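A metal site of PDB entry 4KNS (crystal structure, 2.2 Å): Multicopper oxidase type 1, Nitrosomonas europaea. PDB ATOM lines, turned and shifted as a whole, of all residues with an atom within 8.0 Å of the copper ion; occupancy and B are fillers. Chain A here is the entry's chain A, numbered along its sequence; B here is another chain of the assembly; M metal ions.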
ATOM      1  N   ASP A  62      24.936  -9.689  -0.452  1.00  0.00           N
ATOM      2  CA  ASP A  62      26.055  -8.979   0.156  1.00  0.00           C
ATOM      3  C   ASP A  62      25.507  -7.883   1.069  1.00  0.00           C
ATOM      4  O   ASP A  62      24.804  -6.988   0.609  1.00  0.00           O
ATOM      5  CB  ASP A  62      26.952  -8.384  -0.939  1.00  0.00           C
ATOM      6  CG  ASP A  62      28.093  -7.525  -0.394  1.00  0.00           C
ATOM      7  OD1 ASP A  62      28.003  -7.021   0.749  1.00  0.00           O
ATOM      8  OD2 ASP A  62      29.091  -7.342  -1.122  1.00  0.00           O
ATOM      9  N   PHE A  63      25.819  -7.977   2.356  1.00  0.00           N
ATOM     10  CA  PHE A  63      25.517  -6.913   3.311  1.00  0.00           C
ATOM     11  C   PHE A  63      26.781  -6.124   3.625  1.00  0.00           C
ATOM     12  O   PHE A  63      27.808  -6.713   3.995  1.00  0.00           O
ATOM     13  CB  PHE A  63      24.971  -7.493   4.629  1.00  0.00           C
ATOM     14  CG  PHE A  63      23.517  -7.879   4.579  1.00  0.00           C
ATOM     15  CD1 PHE A  63      22.522  -6.915   4.701  1.00  0.00           C
ATOM     16  CD2 PHE A  63      23.146  -9.211   4.448  1.00  0.00           C
ATOM     17  CE1 PHE A  63      21.176  -7.270   4.670  1.00  0.00           C
ATOM     18  CE2 PHE A  63      21.807  -9.582   4.434  1.00  0.00           C
ATOM     19  CZ  PHE A  63      20.819  -8.603   4.537  1.00  0.00           C
ATOM     20  N   HIS A  64      26.718  -4.800   3.491  1.00  0.00           N
ATOM     21  CA  HIS A  64      27.839  -3.925   3.874  1.00  0.00           C
ATOM     22  C   HIS A  64      28.001  -3.828   5.373  1.00  0.00           C
ATOM     23  O   HIS A  64      29.044  -3.407   5.865  1.00  0.00           O
ATOM     24  CB  HIS A  64      27.698  -2.537   3.262  1.00  0.00           C
ATOM     25  CG  HIS A  64      28.095  -2.466   1.802  1.00  0.00           C
ATOM     26  ND1 HIS A  64      28.615  -1.342   1.256  1.00  0.00           N
ATOM     27  CD2 HIS A  64      28.040  -3.409   0.786  1.00  0.00           C
ATOM     28  CE1 HIS A  64      28.869  -1.578  -0.050  1.00  0.00           C
ATOM     29  NE2 HIS A  64      28.525  -2.837  -0.335  1.00  0.00           N
ATOM     30  N   PHE A  74      28.998 -15.074   0.563  1.00  0.00           N
ATOM     31  CA  PHE A  74      28.335 -14.259  -0.465  1.00  0.00           C
ATOM     32  C   PHE A  74      28.212 -14.979  -1.810  1.00  0.00           C
ATOM     33  O   PHE A  74      27.940 -14.353  -2.830  1.00  0.00           O
ATOM     34  CB  PHE A  74      29.057 -12.907  -0.643  1.00  0.00           C
ATOM     35  CG  PHE A  74      28.981 -11.985   0.545  1.00  0.00           C
ATOM     36  CD1 PHE A  74      28.175 -12.284   1.649  1.00  0.00           C
ATOM     37  CD2 PHE A  74      29.697 -10.797   0.560  1.00  0.00           C
ATOM     38  CE1 PHE A  74      28.103 -11.429   2.734  1.00  0.00           C
ATOM     39  CE2 PHE A  74      29.632  -9.938   1.641  1.00  0.00           C
ATOM     40  CZ  PHE A  74      28.838 -10.243   2.733  1.00  0.00           C
ATOM     41  N   PHE A  96      24.622  -0.277   2.573  1.00  0.00           N
ATOM     42  CA  PHE A  96      24.180  -0.841   1.311  1.00  0.00           C
ATOM     43  C   PHE A  96      24.100  -2.367   1.415  1.00  0.00           C
ATOM     44  O   PHE A  96      25.015  -3.011   1.924  1.00  0.00           O
ATOM     45  CB  PHE A  96      25.174  -0.417   0.222  1.00  0.00           C
ATOM     46  CG  PHE A  96      24.783  -0.807  -1.191  1.00  0.00           C
ATOM     47  CD1 PHE A  96      23.457  -0.964  -1.569  1.00  0.00           C
ATOM     48  CD2 PHE A  96      25.775  -0.959  -2.163  1.00  0.00           C
ATOM     49  CE1 PHE A  96      23.124  -1.311  -2.867  1.00  0.00           C
ATOM     50  CE2 PHE A  96      25.443  -1.292  -3.468  1.00  0.00           C
ATOM     51  CZ  PHE A  96      24.118  -1.479  -3.809  1.00  0.00           C
ATOM     52  N   TYR A  97      22.980  -2.948   0.970  1.00  0.00           N
ATOM     53  CA  TYR A  97      22.962  -4.376   0.675  1.00  0.00           C
ATOM     54  C   TYR A  97      22.532  -4.618  -0.766  1.00  0.00           C
ATOM     55  O   TYR A  97      21.722  -3.868  -1.314  1.00  0.00           O
ATOM     56  CB  TYR A  97      22.143  -5.195   1.702  1.00  0.00           C
ATOM     57  CG  TYR A  97      20.633  -5.233   1.532  1.00  0.00           C
ATOM     58  CD1 TYR A  97      20.041  -5.911   0.458  1.00  0.00           C
ATOM     59  CD2 TYR A  97      19.793  -4.648   2.479  1.00  0.00           C
ATOM     60  CE1 TYR A  97      18.662  -5.964   0.312  1.00  0.00           C
ATOM     61  CE2 TYR A  97      18.415  -4.709   2.348  1.00  0.00           C
ATOM     62  CZ  TYR A  97      17.852  -5.367   1.259  1.00  0.00           C
ATOM     63  OH  TYR A  97      16.489  -5.418   1.120  1.00  0.00           O
ATOM     64  N   HIS A  98      23.087  -5.660  -1.378  1.00  0.00           N
ATOM     65  CA  HIS A  98      22.822  -5.992  -2.777  1.00  0.00           C
ATOM     66  C   HIS A  98      23.212  -7.395  -3.125  1.00  0.00           C
ATOM     67  O   HIS A  98      23.933  -8.053  -2.376  1.00  0.00           O
ATOM     68  CB  HIS A  98      23.557  -5.013  -3.705  1.00  0.00           C
ATOM     69  CG  HIS A  98      25.060  -5.074  -3.576  1.00  0.00           C
ATOM     70  ND1 HIS A  98      25.819  -5.838  -4.387  1.00  0.00           N
ATOM     71  CD2 HIS A  98      25.928  -4.445  -2.696  1.00  0.00           C
ATOM     72  CE1 HIS A  98      27.117  -5.688  -4.045  1.00  0.00           C
ATOM     73  NE2 HIS A  98      27.182  -4.839  -3.009  1.00  0.00           N
ATOM     74  N   CYS A  99      22.743  -7.857  -4.283  1.00  0.00           N
ATOM     75  CA  CYS A  99      23.175  -9.136  -4.835  1.00  0.00           C
ATOM     76  C   CYS A  99      24.614  -9.039  -5.355  1.00  0.00           C
ATOM     77  O   CYS A  99      25.005  -8.023  -5.935  1.00  0.00           O
ATOM     78  CB  CYS A  99      22.239  -9.569  -5.954  1.00  0.00           C
ATOM     79  SG  CYS A  99      22.612 -11.188  -6.658  1.00  0.00           S
ATOM     80  N   GLY A 100      25.387 -10.098  -5.148  1.00  0.00           N
ATOM     81  CA  GLY A 100      26.792 -10.131  -5.553  1.00  0.00           C
ATOM     82  C   GLY A 100      27.129 -11.117  -6.665  1.00  0.00           C
ATOM     83  O   GLY A 100      28.299 -11.463  -6.849  1.00  0.00           O
ATOM     84  N   MET A 104      27.831  -8.447 -11.193  1.00  0.00           N
ATOM     85  CA  MET A 104      27.242  -7.569 -10.168  1.00  0.00           C
ATOM     86  C   MET A 104      26.586  -6.319 -10.751  1.00  0.00           C
ATOM     87  O   MET A 104      25.530  -5.900 -10.288  1.00  0.00           O
ATOM     88  CB  MET A 104      28.286  -7.161  -9.128  1.00  0.00           C
ATOM     89  CG  MET A 104      28.468  -8.172  -8.007  1.00  0.00           C
ATOM     90  SD  MET A 104      29.361  -7.486  -6.594  1.00  0.00           S
ATOM     91  CE  MET A 104      31.058  -7.733  -7.106  1.00  0.00           C
ATOM     92  N   ILE A 108      22.690  -5.504  -9.696  1.00  0.00           N
ATOM     93  CA  ILE A 108      22.320  -4.248  -9.034  1.00  0.00           C
ATOM     94  C   ILE A 108      21.383  -3.423  -9.918  1.00  0.00           C
ATOM     95  O   ILE A 108      20.333  -2.971  -9.450  1.00  0.00           O
ATOM     96  CB  ILE A 108      23.566  -3.422  -8.632  1.00  0.00           C
ATOM     97  CG1 ILE A 108      24.421  -4.198  -7.618  1.00  0.00           C
ATOM     98  CG2 ILE A 108      23.158  -2.062  -8.056  1.00  0.00           C
ATOM     99  CD1 ILE A 108      25.860  -3.715  -7.521  1.00  0.00           C
ATOM    100  N   ASN A 193      23.708   5.045  -2.181  1.00  0.00           N
ATOM    101  CA  ASN A 193      23.956   5.075  -3.624  1.00  0.00           C
ATOM    102  C   ASN A 193      24.288   3.670  -4.129  1.00  0.00           C
ATOM    103  O   ASN A 193      25.422   3.194  -4.006  1.00  0.00           O
ATOM    104  CB  ASN A 193      25.054   6.086  -3.991  1.00  0.00           C
ATOM    105  CG  ASN A 193      25.222   6.258  -5.496  1.00  0.00           C
ATOM    106  OD1 ASN A 193      24.447   5.735  -6.289  1.00  0.00           O
ATOM    107  ND2 ASN A 193      26.253   7.001  -5.889  1.00  0.00           N
ATOM    108  N   ALA A 194      23.270   3.006  -4.691  1.00  0.00           N
ATOM    109  CA  ALA A 194      23.418   1.650  -5.225  1.00  0.00           C
ATOM    110  C   ALA A 194      24.247   1.605  -6.507  1.00  0.00           C
ATOM    111  O   ALA A 194      24.902   0.596  -6.795  1.00  0.00           O
ATOM    112  CB  ALA A 194      22.047   1.035  -5.465  1.00  0.00           C
ATOM    113  N   ALA A 232      29.459   5.451  -5.645  1.00  0.00           N
ATOM    114  CA  ALA A 232      28.771   4.198  -5.916  1.00  0.00           C
ATOM    115  C   ALA A 232      29.118   3.177  -4.847  1.00  0.00           C
ATOM    116  O   ALA A 232      30.286   3.000  -4.501  1.00  0.00           O
ATOM    117  CB  ALA A 232      29.129   3.676  -7.300  1.00  0.00           C
ATOM    118  N   GLY A 233      28.093   2.523  -4.306  1.00  0.00           N
ATOM    119  CA  GLY A 233      28.276   1.521  -3.245  1.00  0.00           C
ATOM    120  C   GLY A 233      28.478   2.116  -1.869  1.00  0.00           C
ATOM    121  O   GLY A 233      28.855   1.407  -0.932  1.00  0.00           O
ATOM    122  N   ASP A 234      28.224   3.414  -1.725  1.00  0.00           N
ATOM    123  CA  ASP A 234      28.367   4.080  -0.437  1.00  0.00           C
ATOM    124  C   ASP A 234      27.016   4.506   0.130  1.00  0.00           C
ATOM    125  O   ASP A 234      26.012   4.535  -0.597  1.00  0.00           O
ATOM    126  CB  ASP A 234      29.307   5.288  -0.548  1.00  0.00           C
ATOM    127  CG  ASP A 234      29.906   5.688   0.793  1.00  0.00           C
ATOM    128  OD1 ASP A 234      29.826   4.890   1.756  1.00  0.00           O
ATOM    129  OD2 ASP A 234      30.462   6.802   0.888  1.00  0.00           O
ATOM    130  N   HIS B 203      35.893  -0.045  -1.625  1.00  0.00           N
ATOM    131  CA  HIS B 203      35.124  -0.824  -0.650  1.00  0.00           C
ATOM    132  C   HIS B 203      35.691  -2.223  -0.496  1.00  0.00           C
ATOM    133  O   HIS B 203      36.049  -2.858  -1.487  1.00  0.00           O
ATOM    134  CB  HIS B 203      33.650  -0.877  -1.069  1.00  0.00           C
ATOM    135  CG  HIS B 203      32.838  -1.933  -0.359  1.00  0.00           C
ATOM    136  ND1 HIS B 203      32.350  -1.753   0.888  1.00  0.00           N
ATOM    137  CD2 HIS B 203      32.425  -3.204  -0.758  1.00  0.00           C
ATOM    138  CE1 HIS B 203      31.666  -2.852   1.265  1.00  0.00           C
ATOM    139  NE2 HIS B 203      31.708  -3.737   0.257  1.00  0.00           N
ATOM    140  N   PRO B 204      35.795  -2.708   0.763  1.00  0.00           N
ATOM    141  CA  PRO B 204      36.187  -4.087   0.990  1.00  0.00           C
ATOM    142  C   PRO B 204      34.959  -5.006   1.090  1.00  0.00           C
ATOM    143  O   PRO B 204      34.242  -4.973   2.095  1.00  0.00           O
ATOM    144  CB  PRO B 204      36.936  -4.022   2.323  1.00  0.00           C
ATOM    145  CG  PRO B 204      36.430  -2.780   3.010  1.00  0.00           C
ATOM    146  CD  PRO B 204      35.589  -1.995   2.034  1.00  0.00           C
ATOM    147  N   ILE B 205      34.728  -5.808   0.056  1.00  0.00           N
ATOM    148  CA  ILE B 205      33.585  -6.729   0.038  1.00  0.00           C
ATOM    149  C   ILE B 205      33.739  -7.769   1.146  1.00  0.00           C
ATOM    150  O   ILE B 205      34.794  -8.391   1.277  1.00  0.00           O
ATOM    151  CB  ILE B 205      33.398  -7.408  -1.346  1.00  0.00           C
ATOM    152  CG1 ILE B 205      33.115  -6.346  -2.415  1.00  0.00           C
ATOM    153  CG2 ILE B 205      32.269  -8.431  -1.296  1.00  0.00           C
ATOM    154  CD1 ILE B 205      32.897  -6.880  -3.817  1.00  0.00           C
ATOM    155  N   ALA B 206      32.679  -7.945   1.940  1.00  0.00           N
ATOM    156  CA  ALA B 206      32.662  -8.812   3.125  1.00  0.00           C
ATOM    157  C   ALA B 206      33.493  -8.254   4.285  1.00  0.00           C
ATOM    158  O   ALA B 206      33.813  -8.980   5.241  1.00  0.00           O
ATOM    159  CB  ALA B 206      33.069 -10.242   2.775  1.00  0.00           C
ATOM    160  N   GLN B 226      32.165   2.073   5.034  1.00  0.00           N
ATOM    161  CA  GLN B 226      31.951   0.975   4.092  1.00  0.00           C
ATOM    162  C   GLN B 226      32.649   1.246   2.754  1.00  0.00           C
ATOM    163  O   GLN B 226      33.155   0.329   2.115  1.00  0.00           O
ATOM    164  CB  GLN B 226      30.463   0.668   3.910  1.00  0.00           C
ATOM    165  CG  GLN B 226      29.654   1.706   3.145  1.00  0.00           C
ATOM    166  CD  GLN B 226      28.163   1.585   3.416  1.00  0.00           C
ATOM    167  OE1 GLN B 226      27.448   0.867   2.704  1.00  0.00           O
ATOM    168  NE2 GLN B 226      27.696   2.262   4.456  1.00  0.00           N
ATOM    169  N   SER B 227      32.670   2.513   2.358  1.00  0.00           N
ATOM    170  CA  SER B 227      33.351   2.941   1.141  1.00  0.00           C
ATOM    171  C   SER B 227      34.040   4.277   1.372  1.00  0.00           C
ATOM    172  O   SER B 227      33.714   5.008   2.322  1.00  0.00           O
ATOM    173  CB  SER B 227      32.351   3.060  -0.025  1.00  0.00           C
ATOM    174  OG  SER B 227      31.762   1.817  -0.321  1.00  0.00           O
ATOM    175  N   VAL B 251      37.432  -3.534  -3.860  1.00  0.00           N
ATOM    176  CA  VAL B 251      36.960  -3.128  -5.184  1.00  0.00           C
ATOM    177  C   VAL B 251      36.741  -1.619  -5.295  1.00  0.00           C
ATOM    178  O   VAL B 251      36.485  -0.937  -4.303  1.00  0.00           O
ATOM    179  CB  VAL B 251      35.645  -3.848  -5.577  1.00  0.00           C
ATOM    180  CG1 VAL B 251      35.839  -5.363  -5.594  1.00  0.00           C
ATOM    181  CG2 VAL B 251      34.495  -3.458  -4.663  1.00  0.00           C
ATOM    182  N   HIS B 253      33.978   0.396  -6.260  1.00  0.00           N
ATOM    183  CA  HIS B 253      32.565  -0.007  -6.255  1.00  0.00           C
ATOM    184  C   HIS B 253      31.751   0.579  -7.389  1.00  0.00           C
ATOM    185  O   HIS B 253      30.593   0.207  -7.564  1.00  0.00           O
ATOM    186  CB  HIS B 253      31.914   0.281  -4.900  1.00  0.00           C
ATOM    187  CG  HIS B 253      30.870  -0.732  -4.511  1.00  0.00           C
ATOM    188  ND1 HIS B 253      29.740  -0.914  -5.223  1.00  0.00           N
ATOM    189  CD2 HIS B 253      30.809  -1.632  -3.447  1.00  0.00           C
ATOM    190  CE1 HIS B 253      28.998  -1.868  -4.644  1.00  0.00           C
ATOM    191  NE2 HIS B 253      29.654  -2.310  -3.567  1.00  0.00           N
ATOM    192  N   MET B 255      30.888  -0.170 -10.471  1.00  0.00           N
ATOM    193  CA  MET B 255      30.979  -1.551 -10.970  1.00  0.00           C
ATOM    194  C   MET B 255      31.637  -1.729 -12.343  1.00  0.00           C
ATOM    195  O   MET B 255      32.255  -2.773 -12.596  1.00  0.00           O
ATOM    196  CB  MET B 255      29.616  -2.264 -10.927  1.00  0.00           C
ATOM    197  CG  MET B 255      29.152  -2.669  -9.529  1.00  0.00           C
ATOM    198  SD  MET B 255      30.381  -3.456  -8.454  1.00  0.00           S
ATOM    199  CE  MET B 255      30.962  -4.822  -9.458  1.00  0.00           C
HETATM  200 CU    CU M   1      28.655  -3.616  -2.246  1.00  0.00          CU
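O of His 98 sits at hydrogen-bond distance from N of Asp 62.
The backbone NH (N) of His 64 is in hydrogen-bond range of the backbone carbonyl oxygen (O) of Phe 96 (2.9 Å).
A ring nitrogen (NE2) of His 64 sits close to a ring nitrogen (NE2) of His 203 of chain B, at 3.4 Å.
A ring nitrogen (ND1) of His 64 is in hydrogen-bond range of the side-chain amide oxygen (OE1) of Gln 226 of chain B, at 2.9 Å.
The backbone NH of Phe 96 is in hydrogen-bond range of the side-chain amide oxygen of Gln 226 of chain B, at 3.1 Å.
The backbone NH (N) of Val 251 of chain B lies within hydrogen-bond range of the backbone carbonyl oxygen (O) of His 203 of chain B (2.8 Å).
O of Gln 226 of chain B is in hydrogen-bond range of ND1 of His 203 of chain B (2.5 Å).
OD2 of Asp 62 touches the copper ion, at 3.9 Å.
CD2 of Phe 96 touches the copper ion, at 3.9 Å.
His 203 of chain B touches the copper ion.
Within 4 Å of the copper ion: Asp 62, His 64, Phe 96, His 98, His 203 of chain B and His 253 of chain B.
The copper ion is bound by NE2 of His 98, NE2 of His 64 and NE2 of His 253 of chain B.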
